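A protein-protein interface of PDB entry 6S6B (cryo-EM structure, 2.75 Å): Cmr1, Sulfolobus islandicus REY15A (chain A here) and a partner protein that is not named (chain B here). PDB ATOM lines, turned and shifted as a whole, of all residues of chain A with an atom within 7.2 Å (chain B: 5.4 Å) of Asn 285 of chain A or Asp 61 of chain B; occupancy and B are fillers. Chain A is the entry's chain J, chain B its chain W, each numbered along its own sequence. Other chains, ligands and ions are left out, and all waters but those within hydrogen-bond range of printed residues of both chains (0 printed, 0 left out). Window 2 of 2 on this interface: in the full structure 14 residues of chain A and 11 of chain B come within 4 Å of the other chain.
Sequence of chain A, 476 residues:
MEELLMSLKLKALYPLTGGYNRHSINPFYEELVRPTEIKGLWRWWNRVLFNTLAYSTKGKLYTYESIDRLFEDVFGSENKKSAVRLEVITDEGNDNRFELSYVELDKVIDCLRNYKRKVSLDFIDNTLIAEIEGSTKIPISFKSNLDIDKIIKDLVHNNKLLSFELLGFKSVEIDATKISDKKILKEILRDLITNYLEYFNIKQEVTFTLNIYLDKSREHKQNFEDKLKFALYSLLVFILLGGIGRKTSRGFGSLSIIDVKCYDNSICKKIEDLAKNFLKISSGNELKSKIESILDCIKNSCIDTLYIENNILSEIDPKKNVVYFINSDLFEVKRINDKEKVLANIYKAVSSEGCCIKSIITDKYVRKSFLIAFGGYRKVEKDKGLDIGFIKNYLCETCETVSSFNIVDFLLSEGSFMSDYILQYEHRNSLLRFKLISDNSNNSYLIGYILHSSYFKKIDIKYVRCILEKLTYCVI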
ATOM      1  N   SER A 282      -7.882 -15.018  -4.262  1.00  0.00           N
ATOM      2  CA  SER A 282      -7.014 -14.992  -3.096  1.00  0.00           C
ATOM      3  C   SER A 282      -5.681 -14.294  -3.315  1.00  0.00           C
ATOM      4  O   SER A 282      -4.860 -14.288  -2.394  1.00  0.00           O
ATOM      5  CB  SER A 282      -6.750 -16.424  -2.606  1.00  0.00           C
ATOM      6  OG  SER A 282      -6.331 -17.253  -3.674  1.00  0.00           O
ATOM      7  N   SER A 283      -5.434 -13.711  -4.485  1.00  0.00           N
ATOM      8  CA  SER A 283      -4.161 -13.054  -4.744  1.00  0.00           C
ATOM      9  C   SER A 283      -4.302 -12.132  -5.943  1.00  0.00           C
ATOM     10  O   SER A 283      -4.986 -12.466  -6.912  1.00  0.00           O
ATOM     11  CB  SER A 283      -3.049 -14.077  -4.988  1.00  0.00           C
ATOM     12  OG  SER A 283      -1.839 -13.434  -5.345  1.00  0.00           O
ATOM     13  N   GLY A 284      -3.643 -10.978  -5.867  1.00  0.00           N
ATOM     14  CA  GLY A 284      -3.705  -9.976  -6.915  1.00  0.00           C
ATOM     15  C   GLY A 284      -3.348 -10.498  -8.290  1.00  0.00           C
ATOM     16  O   GLY A 284      -4.197 -10.543  -9.184  1.00  0.00           O
ATOM     17  N   ASN A 285      -2.092 -10.899  -8.472  1.00  0.00           N
ATOM     18  CA  ASN A 285      -1.667 -11.467  -9.743  1.00  0.00           C
ATOM     19  C   ASN A 285      -2.289 -12.831 -10.023  1.00  0.00           C
ATOM     20  O   ASN A 285      -2.168 -13.326 -11.149  1.00  0.00           O
ATOM     21  CB  ASN A 285      -0.141 -11.548  -9.782  1.00  0.00           C
ATOM     22  CG  ASN A 285       0.431 -12.321  -8.615  1.00  0.00           C
ATOM     23  OD1 ASN A 285      -0.303 -12.895  -7.813  1.00  0.00           O
ATOM     24  ND2 ASN A 285       1.752 -12.335  -8.510  1.00  0.00           N
ATOM     25  N   GLU A 286      -2.946 -13.449  -9.038  1.00  0.00           N
ATOM     26  CA  GLU A 286      -3.715 -14.659  -9.312  1.00  0.00           C
ATOM     27  C   GLU A 286      -4.983 -14.334 -10.085  1.00  0.00           C
ATOM     28  O   GLU A 286      -5.407 -15.108 -10.951  1.00  0.00           O
ATOM     29  CB  GLU A 286      -4.059 -15.372  -8.007  1.00  0.00           C
ATOM     30  CG  GLU A 286      -4.809 -16.674  -8.185  1.00  0.00           C
ATOM     31  CD  GLU A 286      -5.135 -17.344  -6.863  1.00  0.00           C
ATOM     32  OE1 GLU A 286      -4.811 -16.765  -5.805  1.00  0.00           O
ATOM     33  OE2 GLU A 286      -5.712 -18.450  -6.882  1.00  0.00           O
ATOM     34  N   LEU A 287      -5.609 -13.198  -9.776  1.00  0.00           N
ATOM     35  CA  LEU A 287      -6.756 -12.738 -10.549  1.00  0.00           C
ATOM     36  C   LEU A 287      -6.321 -12.196 -11.902  1.00  0.00           C
ATOM     37  O   LEU A 287      -7.034 -12.359 -12.897  1.00  0.00           O
ATOM     38  CB  LEU A 287      -7.520 -11.677  -9.758  1.00  0.00           C
ATOM     39  CG  LEU A 287      -8.523 -10.783 -10.481  1.00  0.00           C
ATOM     40  CD1 LEU A 287      -9.599 -11.612 -11.144  1.00  0.00           C
ATOM     41  CD2 LEU A 287      -9.140  -9.817  -9.491  1.00  0.00           C
ATOM     42  N   LYS A 288      -5.154 -11.548 -11.954  1.00  0.00           N
ATOM     43  CA  LYS A 288      -4.585 -11.137 -13.233  1.00  0.00           C
ATOM     44  C   LYS A 288      -4.437 -12.324 -14.172  1.00  0.00           C
ATOM     45  O   LYS A 288      -4.513 -12.168 -15.397  1.00  0.00           O
ATOM     46  CB  LYS A 288      -3.236 -10.458 -13.000  1.00  0.00           C
ATOM     47  CG  LYS A 288      -2.527 -10.010 -14.262  1.00  0.00           C
ATOM     48  CD  LYS A 288      -3.427  -9.162 -15.130  1.00  0.00           C
ATOM     49  CE  LYS A 288      -2.776  -8.893 -16.472  1.00  0.00           C
ATOM     50  NZ  LYS A 288      -1.498  -8.145 -16.317  1.00  0.00           N
ATOM     51  N   SER A 289      -4.236 -13.520 -13.618  1.00  0.00           N
ATOM     52  CA  SER A 289      -4.272 -14.725 -14.437  1.00  0.00           C
ATOM     53  C   SER A 289      -5.698 -15.066 -14.842  1.00  0.00           C
ATOM     54  O   SER A 289      -5.952 -15.415 -16.000  1.00  0.00           O
ATOM     55  CB  SER A 289      -3.650 -15.894 -13.678  1.00  0.00           C
ATOM     56  OG  SER A 289      -4.600 -16.491 -12.813  1.00  0.00           O
ATOM     57  N   LYS A 290      -6.640 -14.972 -13.901  1.00  0.00           N
ATOM     58  CA  LYS A 290      -8.027 -15.301 -14.210  1.00  0.00           C
ATOM     59  C   LYS A 290      -8.614 -14.331 -15.223  1.00  0.00           C
ATOM     60  O   LYS A 290      -9.332 -14.744 -16.139  1.00  0.00           O
ATOM     61  CB  LYS A 290      -8.861 -15.304 -12.933  1.00  0.00           C
ATOM     62  CG  LYS A 290      -8.582 -16.472 -12.026  1.00  0.00           C
ATOM     63  CD  LYS A 290      -8.961 -16.144 -10.603  1.00  0.00           C
ATOM     64  CE  LYS A 290      -9.006 -17.398  -9.764  1.00  0.00           C
ATOM     65  NZ  LYS A 290      -9.768 -18.469 -10.458  1.00  0.00           N
ATOM     66  N   VAL A 333      -3.895  -5.806 -11.924  1.00  0.00           N
ATOM     67  CA  VAL A 333      -4.687  -6.163 -10.755  1.00  0.00           C
ATOM     68  C   VAL A 333      -3.823  -5.920  -9.526  1.00  0.00           C
ATOM     69  O   VAL A 333      -2.914  -6.703  -9.228  1.00  0.00           O
ATOM     70  CB  VAL A 333      -5.179  -7.611 -10.808  1.00  0.00           C
ATOM     71  CG1 VAL A 333      -6.129  -7.878  -9.660  1.00  0.00           C
ATOM     72  CG2 VAL A 333      -5.853  -7.889 -12.137  1.00  0.00           C
ATOM     73  N   LYS A 334      -4.101  -4.842  -8.811  1.00  0.00           N
ATOM     74  CA  LYS A 334      -3.452  -4.559  -7.547  1.00  0.00           C
ATOM     75  C   LYS A 334      -4.346  -5.033  -6.407  1.00  0.00           C
ATOM     76  O   LYS A 334      -5.352  -5.714  -6.620  1.00  0.00           O
ATOM     77  CB  LYS A 334      -3.134  -3.070  -7.449  1.00  0.00           C
ATOM     78  CG  LYS A 334      -2.244  -2.577  -8.565  1.00  0.00           C
ATOM     79  CD  LYS A 334      -0.976  -3.408  -8.636  1.00  0.00           C
ATOM     80  CE  LYS A 334      -0.169  -3.084  -9.873  1.00  0.00           C
ATOM     81  NZ  LYS A 334      -0.842  -3.558 -11.109  1.00  0.00           N
ATOM     82  N   ARG A 335      -3.975  -4.685  -5.179  1.00  0.00           N
ATOM     83  CA  ARG A 335      -4.786  -4.992  -4.012  1.00  0.00           C
ATOM     84  C   ARG A 335      -5.002  -3.721  -3.208  1.00  0.00           C
ATOM     85  O   ARG A 335      -4.147  -2.833  -3.176  1.00  0.00           O
ATOM     86  CB  ARG A 335      -4.143  -6.069  -3.131  1.00  0.00           C
ATOM     87  CG  ARG A 335      -5.120  -6.741  -2.184  1.00  0.00           C
ATOM     88  CD  ARG A 335      -4.405  -7.407  -1.027  1.00  0.00           C
ATOM     89  NE  ARG A 335      -3.757  -8.647  -1.440  1.00  0.00           N
ATOM     90  CZ  ARG A 335      -4.280  -9.856  -1.271  1.00  0.00           C
ATOM     91  NH1 ARG A 335      -3.619 -10.929  -1.680  1.00  0.00           N
ATOM     92  NH2 ARG A 335      -5.462  -9.994  -0.692  1.00  0.00           N
ATOM     93  N   TYR A 445      -9.545  -5.973  -4.931  1.00  0.00           N
ATOM     94  CA  TYR A 445      -8.520  -5.829  -5.958  1.00  0.00           C
ATOM     95  C   TYR A 445      -8.954  -4.756  -6.941  1.00  0.00           C
ATOM     96  O   TYR A 445      -9.957  -4.922  -7.641  1.00  0.00           O
ATOM     97  CB  TYR A 445      -8.277  -7.144  -6.692  1.00  0.00           C
ATOM     98  CG  TYR A 445      -7.878  -8.289  -5.806  1.00  0.00           C
ATOM     99  CD1 TYR A 445      -6.622  -8.333  -5.221  1.00  0.00           C
ATOM    100  CD2 TYR A 445      -8.748  -9.339  -5.570  1.00  0.00           C
ATOM    101  CE1 TYR A 445      -6.255  -9.380  -4.415  1.00  0.00           C
ATOM    102  CE2 TYR A 445      -8.389 -10.391  -4.767  1.00  0.00           C
ATOM    103  CZ  TYR A 445      -7.143 -10.407  -4.190  1.00  0.00           C
ATOM    104  OH  TYR A 445      -6.786 -11.462  -3.384  1.00  0.00           O
ATOM    105  N   TYR A 473      -0.464   2.168  -9.425  1.00  0.00           N
ATOM    106  CA  TYR A 473       0.361   2.045  -8.232  1.00  0.00           C
ATOM    107  C   TYR A 473       0.117   3.191  -7.256  1.00  0.00           C
ATOM    108  O   TYR A 473      -0.084   2.958  -6.060  1.00  0.00           O
ATOM    109  CB  TYR A 473       1.839   1.980  -8.617  1.00  0.00           C
ATOM    110  CG  TYR A 473       2.332   0.569  -8.824  1.00  0.00           C
ATOM    111  CD1 TYR A 473       2.092  -0.413  -7.875  1.00  0.00           C
ATOM    112  CD2 TYR A 473       3.029   0.216  -9.969  1.00  0.00           C
ATOM    113  CE1 TYR A 473       2.534  -1.704  -8.057  1.00  0.00           C
ATOM    114  CE2 TYR A 473       3.473  -1.074 -10.161  1.00  0.00           C
ATOM    115  CZ  TYR A 473       3.221  -2.030  -9.202  1.00  0.00           C
ATOM    116  OH  TYR A 473       3.660  -3.318  -9.386  1.00  0.00           O
ATOM    117  N   THR B  45       9.134  -2.162  -6.008  1.00  0.00           N
ATOM    118  CA  THR B  45       8.041  -3.118  -6.133  1.00  0.00           C
ATOM    119  C   THR B  45       8.599  -4.529  -6.028  1.00  0.00           C
ATOM    120  O   THR B  45       9.467  -4.916  -6.815  1.00  0.00           O
ATOM    121  CB  THR B  45       7.297  -2.932  -7.454  1.00  0.00           C
ATOM    122  OG1 THR B  45       8.239  -2.814  -8.527  1.00  0.00           O
ATOM    123  CG2 THR B  45       6.441  -1.676  -7.406  1.00  0.00           C
ATOM    124  N   GLY B  46       8.096  -5.291  -5.060  1.00  0.00           N
ATOM    125  CA  GLY B  46       8.562  -6.646  -4.846  1.00  0.00           C
ATOM    126  C   GLY B  46       9.468  -6.780  -3.639  1.00  0.00           C
ATOM    127  O   GLY B  46      10.367  -7.625  -3.625  1.00  0.00           O
ATOM    128  N   THR B  59      11.069  -9.797  -2.935  1.00  0.00           N
ATOM    129  CA  THR B  59      10.071 -10.756  -3.378  1.00  0.00           C
ATOM    130  C   THR B  59       9.853 -10.583  -4.875  1.00  0.00           C
ATOM    131  O   THR B  59      10.355  -9.646  -5.497  1.00  0.00           O
ATOM    132  CB  THR B  59       8.748 -10.576  -2.626  1.00  0.00           C
ATOM    133  OG1 THR B  59       8.025  -9.474  -3.184  1.00  0.00           O
ATOM    134  CG2 THR B  59       9.001 -10.324  -1.154  1.00  0.00           C
ATOM    135  N   LEU B  60       9.086 -11.499  -5.452  1.00  0.00           N
ATOM    136  CA  LEU B  60       8.787 -11.472  -6.874  1.00  0.00           C
ATOM    137  C   LEU B  60       7.285 -11.405  -7.109  1.00  0.00           C
ATOM    138  O   LEU B  60       6.741 -12.066  -7.996  1.00  0.00           O
ATOM    139  CB  LEU B  60       9.403 -12.675  -7.581  1.00  0.00           C
ATOM    140  CG  LEU B  60      10.927 -12.634  -7.705  1.00  0.00           C
ATOM    141  CD1 LEU B  60      11.408 -13.673  -8.698  1.00  0.00           C
ATOM    142  CD2 LEU B  60      11.412 -11.246  -8.104  1.00  0.00           C
ATOM    143  N   ASP B  61       6.596 -10.609  -6.293  1.00  0.00           N
ATOM    144  CA  ASP B  61       5.203 -10.261  -6.523  1.00  0.00           C
ATOM    145  C   ASP B  61       5.135  -8.792  -6.900  1.00  0.00           C
ATOM    146  O   ASP B  61       5.616  -7.946  -6.132  1.00  0.00           O
ATOM    147  CB  ASP B  61       4.358 -10.533  -5.280  1.00  0.00           C
ATOM    148  CG  ASP B  61       2.875 -10.256  -5.499  1.00  0.00           C
ATOM    149  OD1 ASP B  61       2.473  -9.958  -6.642  1.00  0.00           O
ATOM    150  OD2 ASP B  61       2.105 -10.337  -4.519  1.00  0.00           O
ATOM    151  N   PRO B  62       4.579  -8.438  -8.059  1.00  0.00           N
ATOM    152  CA  PRO B  62       4.396  -7.012  -8.373  1.00  0.00           C
ATOM    153  C   PRO B  62       3.498  -6.294  -7.385  1.00  0.00           C
ATOM    154  O   PRO B  62       3.533  -5.059  -7.320  1.00  0.00           O
ATOM    155  CB  PRO B  62       3.782  -7.036  -9.780  1.00  0.00           C
ATOM    156  CG  PRO B  62       3.234  -8.421  -9.941  1.00  0.00           C
ATOM    157  CD  PRO B  62       4.158  -9.306  -9.170  1.00  0.00           C
ATOM    158  N   CYS B  63       2.694  -7.026  -6.611  1.00  0.00           N
ATOM    159  CA  CYS B  63       1.867  -6.436  -5.561  1.00  0.00           C
ATOM    160  C   CYS B  63       2.624  -6.532  -4.239  1.00  0.00           C
ATOM    161  O   CYS B  63       2.322  -7.344  -3.362  1.00  0.00           O
ATOM    162  CB  CYS B  63       0.511  -7.125  -5.495  1.00  0.00           C
ATOM    163  SG  CYS B  63      -0.528  -6.873  -6.950  1.00  0.00           S
ATOM    164  N   ASP B  64       3.637  -5.681  -4.105  1.00  0.00           N
ATOM    165  CA  ASP B  64       4.420  -5.581  -2.877  1.00  0.00           C
ATOM    166  C   ASP B  64       4.906  -4.147  -2.759  1.00  0.00           C
ATOM    167  O   ASP B  64       5.588  -3.649  -3.658  1.00  0.00           O
ATOM    168  CB  ASP B  64       5.597  -6.556  -2.880  1.00  0.00           C
ATOM    169  CG  ASP B  64       5.211  -7.938  -2.403  1.00  0.00           C
ATOM    170  OD1 ASP B  64       4.333  -8.046  -1.522  1.00  0.00           O
ATOM    171  OD2 ASP B  64       5.792  -8.919  -2.912  1.00  0.00           O
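Among the printed residues, merely in contact across the chains: Asn 285 of chain A with Pro 62 of chain B (3.9 Å), Lys 334 of chain A with Cys 63 of chain B (3.8 Å) and Tyr 473 of chain A with Thr 45 of chain B (3.7 Å).
OD1 of Asp 61 of chain B sits at hydrogen-bond distance from ND2 of Asn 285 of chain A (3.1 Å).
The backbone carbonyl oxygen (O) of Val 333 of chain A sits at hydrogen-bond distance from the side-chain sulfur (SG) of Cys 63 of chain B (3.3 Å).
OH of Tyr 473 of chain A is in hydrogen-bond range of O of Pro 62 of chain B, 2.7 Å away.
Printed residues of chain B that touch a printed residue of chain A: Thr 45, Asp 61, Pro 62 and Cys 63.
Along chain B the printed residues that touch a printed residue of chain A span positions 45 to 63.
Printed residues of chain A that touch a printed residue of chain B: Asn 285, Val 333, Lys 334 and Tyr 473.
Hydrophobic or aromatic side chains of chain A within 4 Å of the printed part of chain B: Tyr 473.
Among the printed residues, no Asp or Glu carboxylate lies within 4 Å of a Lys or Arg side-chain nitrogen of the other chain.
OD1 of Asn 285 of chain A sits at hydrogen-bond distance from OG of Ser 283 of chain A (3.0 Å).
The side-chain carboxylate (OD1) of Asp 61 of chain B sits at hydrogen-bond distance from the backbone NH (N) of Cys 63 of chain B (2.9 Å).
Asn 285 of chain A touches two residues of chain B.
Of chain A, only Asn 285 comes within 4 Å of Asp 61 of chain B.
Of the printed residues of chain B, Lys 334 of chain A touches Cys 63 (3.8 Å).
Of the printed residues of chain B, Val 333 of chain A touches Cys 63 (3.3 Å).
Printed residues of chain A within 4 Å of Cys 63 of chain B: Val 333 and Lys 334.
Of the printed residues of chain A, Pro 62 of chain B touches Asn 285 (3.9 Å) and Tyr 473 (2.7 Å).
Printed residues of chain B within 4 Å of Tyr 473 of chain A: Thr 45 (3.7 Å) and Pro 62 (2.7 Å).
Ser 282 of chain A touches none of the printed residues of chain B.
Thr 59 of chain B touches none of the printed residues of chain A.
The nearest printed residue of chain A that does not touch Pro 62 of chain B is Lys 334 of chain A (4.9 Å).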
